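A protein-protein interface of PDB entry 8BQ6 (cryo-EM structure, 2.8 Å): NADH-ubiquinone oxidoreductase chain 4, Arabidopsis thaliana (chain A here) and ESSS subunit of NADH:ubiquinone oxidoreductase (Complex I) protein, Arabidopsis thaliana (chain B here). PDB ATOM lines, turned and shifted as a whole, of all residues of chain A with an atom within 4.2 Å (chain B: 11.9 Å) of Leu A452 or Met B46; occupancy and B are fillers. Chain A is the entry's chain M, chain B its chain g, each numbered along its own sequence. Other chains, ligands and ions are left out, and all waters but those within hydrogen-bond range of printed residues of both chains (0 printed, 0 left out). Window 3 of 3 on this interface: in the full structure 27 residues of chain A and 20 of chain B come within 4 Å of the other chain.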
ATOM      1  N   VAL A 354     -17.785  -4.020  33.821  1.00  0.00           N
ATOM      2  CA  VAL A 354     -17.327  -4.126  32.438  1.00  0.00           C
ATOM      3  C   VAL A 354     -16.863  -2.768  31.929  1.00  0.00           C
ATOM      4  O   VAL A 354     -15.803  -2.651  31.303  1.00  0.00           O
ATOM      5  CB  VAL A 354     -18.441  -4.720  31.554  1.00  0.00           C
ATOM      6  CG1 VAL A 354     -18.332  -4.205  30.129  1.00  0.00           C
ATOM      7  CG2 VAL A 354     -18.370  -6.232  31.567  1.00  0.00           C
ATOM      8  N   ARG A 358     -12.329  -1.242  31.627  1.00  0.00           N
ATOM      9  CA  ARG A 358     -11.757  -0.681  30.411  1.00  0.00           C
ATOM     10  C   ARG A 358     -11.361   0.781  30.574  1.00  0.00           C
ATOM     11  O   ARG A 358     -10.233   1.159  30.247  1.00  0.00           O
ATOM     12  CB  ARG A 358     -12.740  -0.812  29.246  1.00  0.00           C
ATOM     13  CG  ARG A 358     -13.040  -2.226  28.833  1.00  0.00           C
ATOM     14  CD  ARG A 358     -14.418  -2.308  28.230  1.00  0.00           C
ATOM     15  NE  ARG A 358     -14.605  -3.535  27.470  1.00  0.00           N
ATOM     16  CZ  ARG A 358     -14.785  -4.729  28.012  1.00  0.00           C
ATOM     17  NH1 ARG A 358     -14.809  -4.895  29.325  1.00  0.00           N
ATOM     18  NH2 ARG A 358     -14.945  -5.783  27.220  1.00  0.00           N
ATOM     19  N   ASN A 376     -23.375  -5.084  21.856  1.00  0.00           N
ATOM     20  CA  ASN A 376     -23.657  -6.279  22.646  1.00  0.00           C
ATOM     21  C   ASN A 376     -23.845  -5.937  24.116  1.00  0.00           C
ATOM     22  O   ASN A 376     -24.786  -6.414  24.760  1.00  0.00           O
ATOM     23  CB  ASN A 376     -22.535  -7.301  22.487  1.00  0.00           C
ATOM     24  CG  ASN A 376     -22.680  -8.123  21.239  1.00  0.00           C
ATOM     25  OD1 ASN A 376     -23.776  -8.269  20.707  1.00  0.00           O
ATOM     26  ND2 ASN A 376     -21.575  -8.681  20.766  1.00  0.00           N
ATOM     27  N   PHE A 377     -22.944  -5.123  24.666  1.00  0.00           N
ATOM     28  CA  PHE A 377     -23.092  -4.677  26.045  1.00  0.00           C
ATOM     29  C   PHE A 377     -24.354  -3.844  26.213  1.00  0.00           C
ATOM     30  O   PHE A 377     -25.061  -3.969  27.219  1.00  0.00           O
ATOM     31  CB  PHE A 377     -21.848  -3.891  26.465  1.00  0.00           C
ATOM     32  CG  PHE A 377     -22.038  -3.045  27.693  1.00  0.00           C
ATOM     33  CD1 PHE A 377     -21.891  -3.590  28.954  1.00  0.00           C
ATOM     34  CD2 PHE A 377     -22.335  -1.699  27.583  1.00  0.00           C
ATOM     35  CE1 PHE A 377     -22.057  -2.816  30.081  1.00  0.00           C
ATOM     36  CE2 PHE A 377     -22.504  -0.922  28.708  1.00  0.00           C
ATOM     37  CZ  PHE A 377     -22.359  -1.481  29.959  1.00  0.00           C
ATOM     38  N   ILE A 380     -27.445  -6.187  26.470  1.00  0.00           N
ATOM     39  CA  ILE A 380     -27.456  -6.867  27.762  1.00  0.00           C
ATOM     40  C   ILE A 380     -27.742  -5.877  28.883  1.00  0.00           C
ATOM     41  O   ILE A 380     -28.471  -6.182  29.835  1.00  0.00           O
ATOM     42  CB  ILE A 380     -26.121  -7.607  27.974  1.00  0.00           C
ATOM     43  CG1 ILE A 380     -26.059  -8.848  27.082  1.00  0.00           C
ATOM     44  CG2 ILE A 380     -25.908  -7.969  29.433  1.00  0.00           C
ATOM     45  CD1 ILE A 380     -24.737  -9.554  27.108  1.00  0.00           C
ATOM     46  N   ASP A 451     -16.059  -4.154  22.866  1.00  0.00           N
ATOM     47  CA  ASP A 451     -17.269  -4.798  23.342  1.00  0.00           C
ATOM     48  C   ASP A 451     -16.908  -6.002  24.208  1.00  0.00           C
ATOM     49  O   ASP A 451     -15.736  -6.300  24.455  1.00  0.00           O
ATOM     50  CB  ASP A 451     -18.147  -5.211  22.166  1.00  0.00           C
ATOM     51  CG  ASP A 451     -19.623  -5.120  22.481  1.00  0.00           C
ATOM     52  OD1 ASP A 451     -19.976  -5.117  23.677  1.00  0.00           O
ATOM     53  OD2 ASP A 451     -20.430  -5.043  21.536  1.00  0.00           O
ATOM     54  N   LEU A 452     -17.935  -6.710  24.666  1.00  0.00           N
ATOM     55  CA  LEU A 452     -17.715  -7.844  25.548  1.00  0.00           C
ATOM     56  C   LEU A 452     -16.927  -8.936  24.845  1.00  0.00           C
ATOM     57  O   LEU A 452     -17.065  -9.148  23.637  1.00  0.00           O
ATOM     58  CB  LEU A 452     -19.044  -8.406  26.039  1.00  0.00           C
ATOM     59  CG  LEU A 452     -20.065  -7.389  26.530  1.00  0.00           C
ATOM     60  CD1 LEU A 452     -21.412  -8.052  26.651  1.00  0.00           C
ATOM     61  CD2 LEU A 452     -19.625  -6.811  27.858  1.00  0.00           C
ATOM     62  N   ASN A 453     -16.089  -9.624  25.609  1.00  0.00           N
ATOM     63  CA  ASN A 453     -15.383 -10.778  25.087  1.00  0.00           C
ATOM     64  C   ASN A 453     -16.130 -12.055  25.464  1.00  0.00           C
ATOM     65  O   ASN A 453     -17.219 -12.024  26.044  1.00  0.00           O
ATOM     66  CB  ASN A 453     -13.938 -10.793  25.583  1.00  0.00           C
ATOM     67  CG  ASN A 453     -13.829 -10.747  27.098  1.00  0.00           C
ATOM     68  OD1 ASN A 453     -14.389 -11.582  27.805  1.00  0.00           O
ATOM     69  ND2 ASN A 453     -13.083  -9.775  27.600  1.00  0.00           N
ATOM     70  N   GLY A 454     -15.528 -13.195  25.129  1.00  0.00           N
ATOM     71  CA  GLY A 454     -16.195 -14.468  25.349  1.00  0.00           C
ATOM     72  C   GLY A 454     -16.464 -14.756  26.814  1.00  0.00           C
ATOM     73  O   GLY A 454     -17.466 -15.388  27.156  1.00  0.00           O
ATOM     74  N   GLU A 456     -17.030 -12.487  29.241  1.00  0.00           N
ATOM     75  CA  GLU A 456     -18.068 -11.612  29.774  1.00  0.00           C
ATOM     76  C   GLU A 456     -19.451 -12.009  29.273  1.00  0.00           C
ATOM     77  O   GLU A 456     -20.432 -11.922  30.019  1.00  0.00           O
ATOM     78  CB  GLU A 456     -17.771 -10.160  29.414  1.00  0.00           C
ATOM     79  CG  GLU A 456     -16.739  -9.504  30.302  1.00  0.00           C
ATOM     80  CD  GLU A 456     -15.927  -8.464  29.566  1.00  0.00           C
ATOM     81  OE1 GLU A 456     -15.645  -7.398  30.149  1.00  0.00           O
ATOM     82  OE2 GLU A 456     -15.566  -8.711  28.400  1.00  0.00           O
ATOM     83  N   VAL A 457     -19.554 -12.431  28.012  1.00  0.00           N
ATOM     84  CA  VAL A 457     -20.844 -12.877  27.495  1.00  0.00           C
ATOM     85  C   VAL A 457     -21.308 -14.118  28.243  1.00  0.00           C
ATOM     86  O   VAL A 457     -22.465 -14.210  28.673  1.00  0.00           O
ATOM     87  CB  VAL A 457     -20.765 -13.129  25.979  1.00  0.00           C
ATOM     88  CG1 VAL A 457     -21.954 -13.946  25.522  1.00  0.00           C
ATOM     89  CG2 VAL A 457     -20.707 -11.813  25.229  1.00  0.00           C
ATOM     90  N   PRO B  41     -19.191 -10.391   7.419  1.00  0.00           N
ATOM     91  CA  PRO B  41     -19.859  -9.419   8.290  1.00  0.00           C
ATOM     92  C   PRO B  41     -18.871  -8.462   8.941  1.00  0.00           C
ATOM     93  O   PRO B  41     -17.694  -8.766   9.145  1.00  0.00           O
ATOM     94  CB  PRO B  41     -20.554 -10.297   9.333  1.00  0.00           C
ATOM     95  CG  PRO B  41     -20.671 -11.633   8.698  1.00  0.00           C
ATOM     96  CD  PRO B  41     -19.464 -11.777   7.829  1.00  0.00           C
ATOM     97  N   LYS B  42     -19.378  -7.271   9.253  1.00  0.00           N
ATOM     98  CA  LYS B  42     -18.576  -6.247   9.905  1.00  0.00           C
ATOM     99  C   LYS B  42     -18.320  -6.618  11.362  1.00  0.00           C
ATOM    100  O   LYS B  42     -19.225  -7.057  12.077  1.00  0.00           O
ATOM    101  CB  LYS B  42     -19.264  -4.882   9.804  1.00  0.00           C
ATOM    102  CG  LYS B  42     -20.745  -4.882  10.145  1.00  0.00           C
ATOM    103  CD  LYS B  42     -21.247  -3.478  10.455  1.00  0.00           C
ATOM    104  CE  LYS B  42     -21.562  -2.675   9.200  1.00  0.00           C
ATOM    105  NZ  LYS B  42     -22.828  -3.122   8.560  1.00  0.00           N
ATOM    106  N   GLY B  43     -17.069  -6.460  11.788  1.00  0.00           N
ATOM    107  CA  GLY B  43     -16.678  -6.805  13.139  1.00  0.00           C
ATOM    108  C   GLY B  43     -16.461  -8.294  13.318  1.00  0.00           C
ATOM    109  O   GLY B  43     -16.581  -9.101  12.395  1.00  0.00           O
ATOM    110  N   TYR B  44     -16.129  -8.661  14.551  1.00  0.00           N
ATOM    111  CA  TYR B  44     -15.917 -10.052  14.917  1.00  0.00           C
ATOM    112  C   TYR B  44     -16.727 -10.377  16.159  1.00  0.00           C
ATOM    113  O   TYR B  44     -16.840  -9.555  17.073  1.00  0.00           O
ATOM    114  CB  TYR B  44     -14.440 -10.347  15.157  1.00  0.00           C
ATOM    115  CG  TYR B  44     -13.663 -10.358  13.874  1.00  0.00           C
ATOM    116  CD1 TYR B  44     -14.084 -11.128  12.803  1.00  0.00           C
ATOM    117  CD2 TYR B  44     -12.533  -9.573  13.717  1.00  0.00           C
ATOM    118  CE1 TYR B  44     -13.395 -11.132  11.620  1.00  0.00           C
ATOM    119  CE2 TYR B  44     -11.835  -9.568  12.533  1.00  0.00           C
ATOM    120  CZ  TYR B  44     -12.270 -10.353  11.489  1.00  0.00           C
ATOM    121  OH  TYR B  44     -11.585 -10.363  10.299  1.00  0.00           O
ATOM    122  N   PHE B  45     -17.288 -11.579  16.175  1.00  0.00           N
ATOM    123  CA  PHE B  45     -18.140 -12.005  17.273  1.00  0.00           C
ATOM    124  C   PHE B  45     -17.336 -12.124  18.559  1.00  0.00           C
ATOM    125  O   PHE B  45     -16.406 -12.932  18.647  1.00  0.00           O
ATOM    126  CB  PHE B  45     -18.791 -13.336  16.924  1.00  0.00           C
ATOM    127  CG  PHE B  45     -19.735 -13.832  17.962  1.00  0.00           C
ATOM    128  CD1 PHE B  45     -20.769 -13.035  18.409  1.00  0.00           C
ATOM    129  CD2 PHE B  45     -19.580 -15.091  18.505  1.00  0.00           C
ATOM    130  CE1 PHE B  45     -21.636 -13.490  19.372  1.00  0.00           C
ATOM    131  CE2 PHE B  45     -20.449 -15.552  19.462  1.00  0.00           C
ATOM    132  CZ  PHE B  45     -21.476 -14.750  19.900  1.00  0.00           C
ATOM    133  N   MET B  46     -17.716 -11.328  19.560  1.00  0.00           N
ATOM    134  CA  MET B  46     -16.993 -11.224  20.828  1.00  0.00           C
ATOM    135  C   MET B  46     -15.600 -10.631  20.636  1.00  0.00           C
ATOM    136  O   MET B  46     -14.713 -10.834  21.467  1.00  0.00           O
ATOM    137  CB  MET B  46     -16.910 -12.573  21.551  1.00  0.00           C
ATOM    138  CG  MET B  46     -18.258 -13.170  21.916  1.00  0.00           C
ATOM    139  SD  MET B  46     -18.257 -14.970  21.959  1.00  0.00           S
ATOM    140  CE  MET B  46     -19.782 -15.269  22.847  1.00  0.00           C
ATOM    141  N   ASN B  47     -15.408  -9.891  19.540  1.00  0.00           N
ATOM    142  CA  ASN B  47     -14.186  -9.123  19.275  1.00  0.00           C
ATOM    143  C   ASN B  47     -12.922  -9.970  19.349  1.00  0.00           C
ATOM    144  O   ASN B  47     -11.882  -9.505  19.822  1.00  0.00           O
ATOM    145  CB  ASN B  47     -14.051  -7.929  20.221  1.00  0.00           C
ATOM    146  CG  ASN B  47     -14.975  -6.796  19.863  1.00  0.00           C
ATOM    147  OD1 ASN B  47     -16.045  -7.007  19.294  1.00  0.00           O
ATOM    148  ND2 ASN B  47     -14.563  -5.578  20.186  1.00  0.00           N
ATOM    149  N   ARG B  48     -12.980 -11.207  18.879  1.00  0.00           N
ATOM    150  CA  ARG B  48     -11.798 -12.047  18.796  1.00  0.00           C
ATOM    151  C   ARG B  48     -11.404 -12.193  17.335  1.00  0.00           C
ATOM    152  O   ARG B  48     -12.231 -12.568  16.498  1.00  0.00           O
ATOM    153  CB  ARG B  48     -12.043 -13.413  19.435  1.00  0.00           C
ATOM    154  CG  ARG B  48     -12.224 -13.375  20.932  1.00  0.00           C
ATOM    155  CD  ARG B  48     -12.627 -14.737  21.440  1.00  0.00           C
ATOM    156  NE  ARG B  48     -13.925 -15.149  20.922  1.00  0.00           N
ATOM    157  CZ  ARG B  48     -14.504 -16.304  21.219  1.00  0.00           C
ATOM    158  NH1 ARG B  48     -13.931 -17.171  22.035  1.00  0.00           N
ATOM    159  NH2 ARG B  48     -15.689 -16.592  20.687  1.00  0.00           N
ATOM    160  N   THR B  49     -10.151 -11.868  17.030  1.00  0.00           N
ATOM    161  CA  THR B  49      -9.648 -12.068  15.684  1.00  0.00           C
ATOM    162  C   THR B  49      -9.712 -13.552  15.334  1.00  0.00           C
ATOM    163  O   THR B  49      -9.425 -14.406  16.176  1.00  0.00           O
ATOM    164  CB  THR B  49      -8.211 -11.575  15.564  1.00  0.00           C
ATOM    165  OG1 THR B  49      -7.406 -12.217  16.561  1.00  0.00           O
ATOM    166  CG2 THR B  49      -8.143 -10.071  15.766  1.00  0.00           C
ATOM    167  N   PRO B  50     -10.106 -13.887  14.111  1.00  0.00           N
ATOM    168  CA  PRO B  50     -10.162 -15.290  13.715  1.00  0.00           C
ATOM    169  C   PRO B  50      -8.776 -15.906  13.700  1.00  0.00           C
ATOM    170  O   PRO B  50      -7.771 -15.200  13.532  1.00  0.00           O
ATOM    171  CB  PRO B  50     -10.772 -15.224  12.307  1.00  0.00           C
ATOM    172  CG  PRO B  50     -10.320 -13.897  11.804  1.00  0.00           C
ATOM    173  CD  PRO B  50     -10.539 -13.013  13.008  1.00  0.00           C
ATOM    174  N   PRO B  51      -8.679 -17.217  13.897  1.00  0.00           N
ATOM    175  CA  PRO B  51      -7.369 -17.873  13.865  1.00  0.00           C
ATOM    176  C   PRO B  51      -6.840 -17.977  12.443  1.00  0.00           C
ATOM    177  O   PRO B  51      -7.529 -17.669  11.468  1.00  0.00           O
ATOM    178  CB  PRO B  51      -7.646 -19.257  14.461  1.00  0.00           C
ATOM    179  CG  PRO B  51      -9.129 -19.465  14.339  1.00  0.00           C
ATOM    180  CD  PRO B  51      -9.791 -18.179  13.950  1.00  0.00           C
ATOM    181  N   ARG B  57      -9.420 -22.265  16.987  1.00  0.00           N
ATOM    182  CA  ARG B  57      -9.231 -21.337  18.093  1.00  0.00           C
ATOM    183  C   ARG B  57      -8.809 -22.089  19.347  1.00  0.00           C
ATOM    184  O   ARG B  57      -9.267 -23.204  19.607  1.00  0.00           O
ATOM    185  CB  ARG B  57     -10.517 -20.547  18.346  1.00  0.00           C
ATOM    186  CG  ARG B  57     -10.453 -19.588  19.530  1.00  0.00           C
ATOM    187  CD  ARG B  57     -11.774 -18.852  19.743  1.00  0.00           C
ATOM    188  NE  ARG B  57     -12.835 -19.696  20.280  1.00  0.00           N
ATOM    189  CZ  ARG B  57     -13.052 -19.894  21.573  1.00  0.00           C
ATOM    190  NH1 ARG B  57     -12.233 -19.409  22.492  1.00  0.00           N
ATOM    191  NH2 ARG B  57     -14.119 -20.591  21.953  1.00  0.00           N
ATOM    192  N   LYS B  58      -7.903 -21.489  20.110  1.00  0.00           N
ATOM    193  CA  LYS B  58      -7.524 -22.059  21.392  1.00  0.00           C
ATOM    194  C   LYS B  58      -8.595 -21.721  22.415  1.00  0.00           C
ATOM    195  O   LYS B  58      -9.009 -20.565  22.533  1.00  0.00           O
ATOM    196  CB  LYS B  58      -6.171 -21.521  21.846  1.00  0.00           C
ATOM    197  CG  LYS B  58      -5.002 -22.000  21.013  1.00  0.00           C
ATOM    198  CD  LYS B  58      -3.720 -21.307  21.437  1.00  0.00           C
ATOM    199  CE  LYS B  58      -3.333 -21.684  22.856  1.00  0.00           C
ATOM    200  NZ  LYS B  58      -2.015 -21.102  23.232  1.00  0.00           N
ATOM    201  N   TRP B  59      -9.059 -22.728  23.141  1.00  0.00           N
ATOM    202  CA  TRP B  59      -9.999 -22.475  24.218  1.00  0.00           C
ATOM    203  C   TRP B  59      -9.235 -21.967  25.427  1.00  0.00           C
ATOM    204  O   TRP B  59      -8.158 -22.476  25.753  1.00  0.00           O
ATOM    205  CB  TRP B  59     -10.777 -23.737  24.571  1.00  0.00           C
ATOM    206  CG  TRP B  59     -11.913 -24.005  23.652  1.00  0.00           C
ATOM    207  CD1 TRP B  59     -12.106 -23.478  22.410  1.00  0.00           C
ATOM    208  CD2 TRP B  59     -13.012 -24.884  23.890  1.00  0.00           C
ATOM    209  NE1 TRP B  59     -13.264 -23.972  21.862  1.00  0.00           N
ATOM    210  CE2 TRP B  59     -13.837 -24.841  22.752  1.00  0.00           C
ATOM    211  CE3 TRP B  59     -13.378 -25.707  24.956  1.00  0.00           C
ATOM    212  CZ2 TRP B  59     -15.007 -25.583  22.653  1.00  0.00           C
ATOM    213  CZ3 TRP B  59     -14.535 -26.441  24.856  1.00  0.00           C
ATOM    214  CH2 TRP B  59     -15.337 -26.375  23.714  1.00  0.00           C
ATOM    215  N   GLU B  60      -9.776 -20.947  26.076  1.00  0.00           N
ATOM    216  CA  GLU B  60      -9.205 -20.508  27.331  1.00  0.00           C
ATOM    217  C   GLU B  60      -9.466 -21.551  28.409  1.00  0.00           C
ATOM    218  O   GLU B  60     -10.285 -22.459  28.249  1.00  0.00           O
ATOM    219  CB  GLU B  60      -9.778 -19.156  27.724  1.00  0.00           C
ATOM    220  CG  GLU B  60      -9.570 -18.125  26.651  1.00  0.00           C
ATOM    221  CD  GLU B  60      -9.470 -16.735  27.208  1.00  0.00           C
ATOM    222  OE1 GLU B  60     -10.400 -16.318  27.929  1.00  0.00           O
ATOM    223  OE2 GLU B  60      -8.460 -16.060  26.930  1.00  0.00           O
ATOM    224  N   TRP B  62     -10.903 -21.500  31.220  1.00  0.00           N
ATOM    225  CA  TRP B  62     -12.180 -21.528  31.918  1.00  0.00           C
ATOM    226  C   TRP B  62     -13.296 -22.165  31.098  1.00  0.00           C
ATOM    227  O   TRP B  62     -14.302 -22.581  31.681  1.00  0.00           O
ATOM    228  CB  TRP B  62     -12.575 -20.108  32.323  1.00  0.00           C
ATOM    229  CG  TRP B  62     -12.631 -19.182  31.163  1.00  0.00           C
ATOM    230  CD1 TRP B  62     -11.630 -18.376  30.714  1.00  0.00           C
ATOM    231  CD2 TRP B  62     -13.746 -18.963  30.293  1.00  0.00           C
ATOM    232  NE1 TRP B  62     -12.049 -17.670  29.615  1.00  0.00           N
ATOM    233  CE2 TRP B  62     -13.345 -18.013  29.336  1.00  0.00           C
ATOM    234  CE3 TRP B  62     -15.041 -19.477  30.231  1.00  0.00           C
ATOM    235  CZ2 TRP B  62     -14.193 -17.570  28.329  1.00  0.00           C
ATOM    236  CZ3 TRP B  62     -15.879 -19.038  29.232  1.00  0.00           C
ATOM    237  CH2 TRP B  62     -15.454 -18.093  28.294  1.00  0.00           C
ATOM    238  N   GLU B  63     -13.138 -22.269  29.777  1.00  0.00           N
ATOM    239  CA  GLU B  63     -14.255 -22.651  28.915  1.00  0.00           C
ATOM    240  C   GLU B  63     -14.737 -24.068  29.204  1.00  0.00           C
ATOM    241  O   GLU B  63     -15.933 -24.299  29.406  1.00  0.00           O
ATOM    242  CB  GLU B  63     -13.856 -22.515  27.448  1.00  0.00           C
ATOM    243  CG  GLU B  63     -13.077 -21.269  27.148  1.00  0.00           C
ATOM    244  CD  GLU B  63     -13.451 -20.678  25.821  1.00  0.00           C
ATOM    245  OE1 GLU B  63     -14.640 -20.766  25.452  1.00  0.00           O
ATOM    246  OE2 GLU B  63     -12.562 -20.122  25.148  1.00  0.00           O
ATOM    247  N   TYR B  67     -18.344 -24.978  30.419  1.00  0.00           N
ATOM    248  CA  TYR B  67     -19.293 -25.576  29.483  1.00  0.00           C
ATOM    249  C   TYR B  67     -19.733 -26.956  29.948  1.00  0.00           C
ATOM    250  O   TYR B  67     -20.761 -27.471  29.496  1.00  0.00           O
ATOM    251  CB  TYR B  67     -18.697 -25.659  28.081  1.00  0.00           C
ATOM    252  CG  TYR B  67     -18.336 -24.324  27.489  1.00  0.00           C
ATOM    253  CD1 TYR B  67     -18.940 -23.158  27.933  1.00  0.00           C
ATOM    254  CD2 TYR B  67     -17.393 -24.232  26.481  1.00  0.00           C
ATOM    255  CE1 TYR B  67     -18.607 -21.939  27.393  1.00  0.00           C
ATOM    256  CE2 TYR B  67     -17.059 -23.021  25.933  1.00  0.00           C
ATOM    257  CZ  TYR B  67     -17.665 -21.878  26.392  1.00  0.00           C
ATOM    258  OH  TYR B  67     -17.326 -20.666  25.842  1.00  0.00           O
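The backbone NH (N) of Asp A451 lies close to the side-chain amide nitrogen (ND2) of Asn B47, at 3.4 Å.
No residue of chain B comes within 4 Å of Val A354.
No residue of chain B comes within 4 Å of Asn A376.
No residue of chain B comes within 4 Å of Phe A377.
Of chain B, only Met B46 comes within 4 Å of Leu A452.
Of chain B, only Met B46 comes within 4 Å of Asn A453.
Gly A454 touches two residues of chain B.
Glu A456 touches none of the printed residues of chain B.
Printed residues of chain A within 4 Å of Asn B47: Asp A451.
Printed residues of chain A within 4 Å of Trp B62: Gly A454 (3.6 Å).
The nearest residue of chain B that does not touch Leu A452 is Asn B47 (4.5 Å).
The nearest printed residue of chain A that does not touch Met B46 is Asn A376 (4.8 Å).
The backbone NH (N) of Asn A376 sits at hydrogen-bond distance from the side-chain carboxylate (OD2) of Asp A451 (3.0 Å).
The guanidinium group of Arg B48 is in hydrogen-bond range of the side-chain sulfur of Met B46.
O of Tyr B44 sits close to OD1 of Asn B47 (3.5 Å).
The side-chain carboxylate (OE2) of Glu A456 is in hydrogen-bond range of the side-chain amide nitrogen (ND2) of Asn A453 (2.8 Å).
O of Asp A451 sits at hydrogen-bond distance from NH2 of Arg A358.
The backbone NH (N) of Phe A377 sits at hydrogen-bond distance from the side-chain carboxylate (OD1) of Asp A451 (3.1 Å).
Among the printed residues, 6 pairs touch across the chains.
Leu A452 touches Met B46 (O to CA, 3.5 Å).
Asn A453 touches Met B46.
Met B46 touches Gly A454 (CB to N, 3.9 Å).
Gly A454 touches Trp B62.
Met B46 touches Val A457 (CE to CG1, 3.7 Å).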
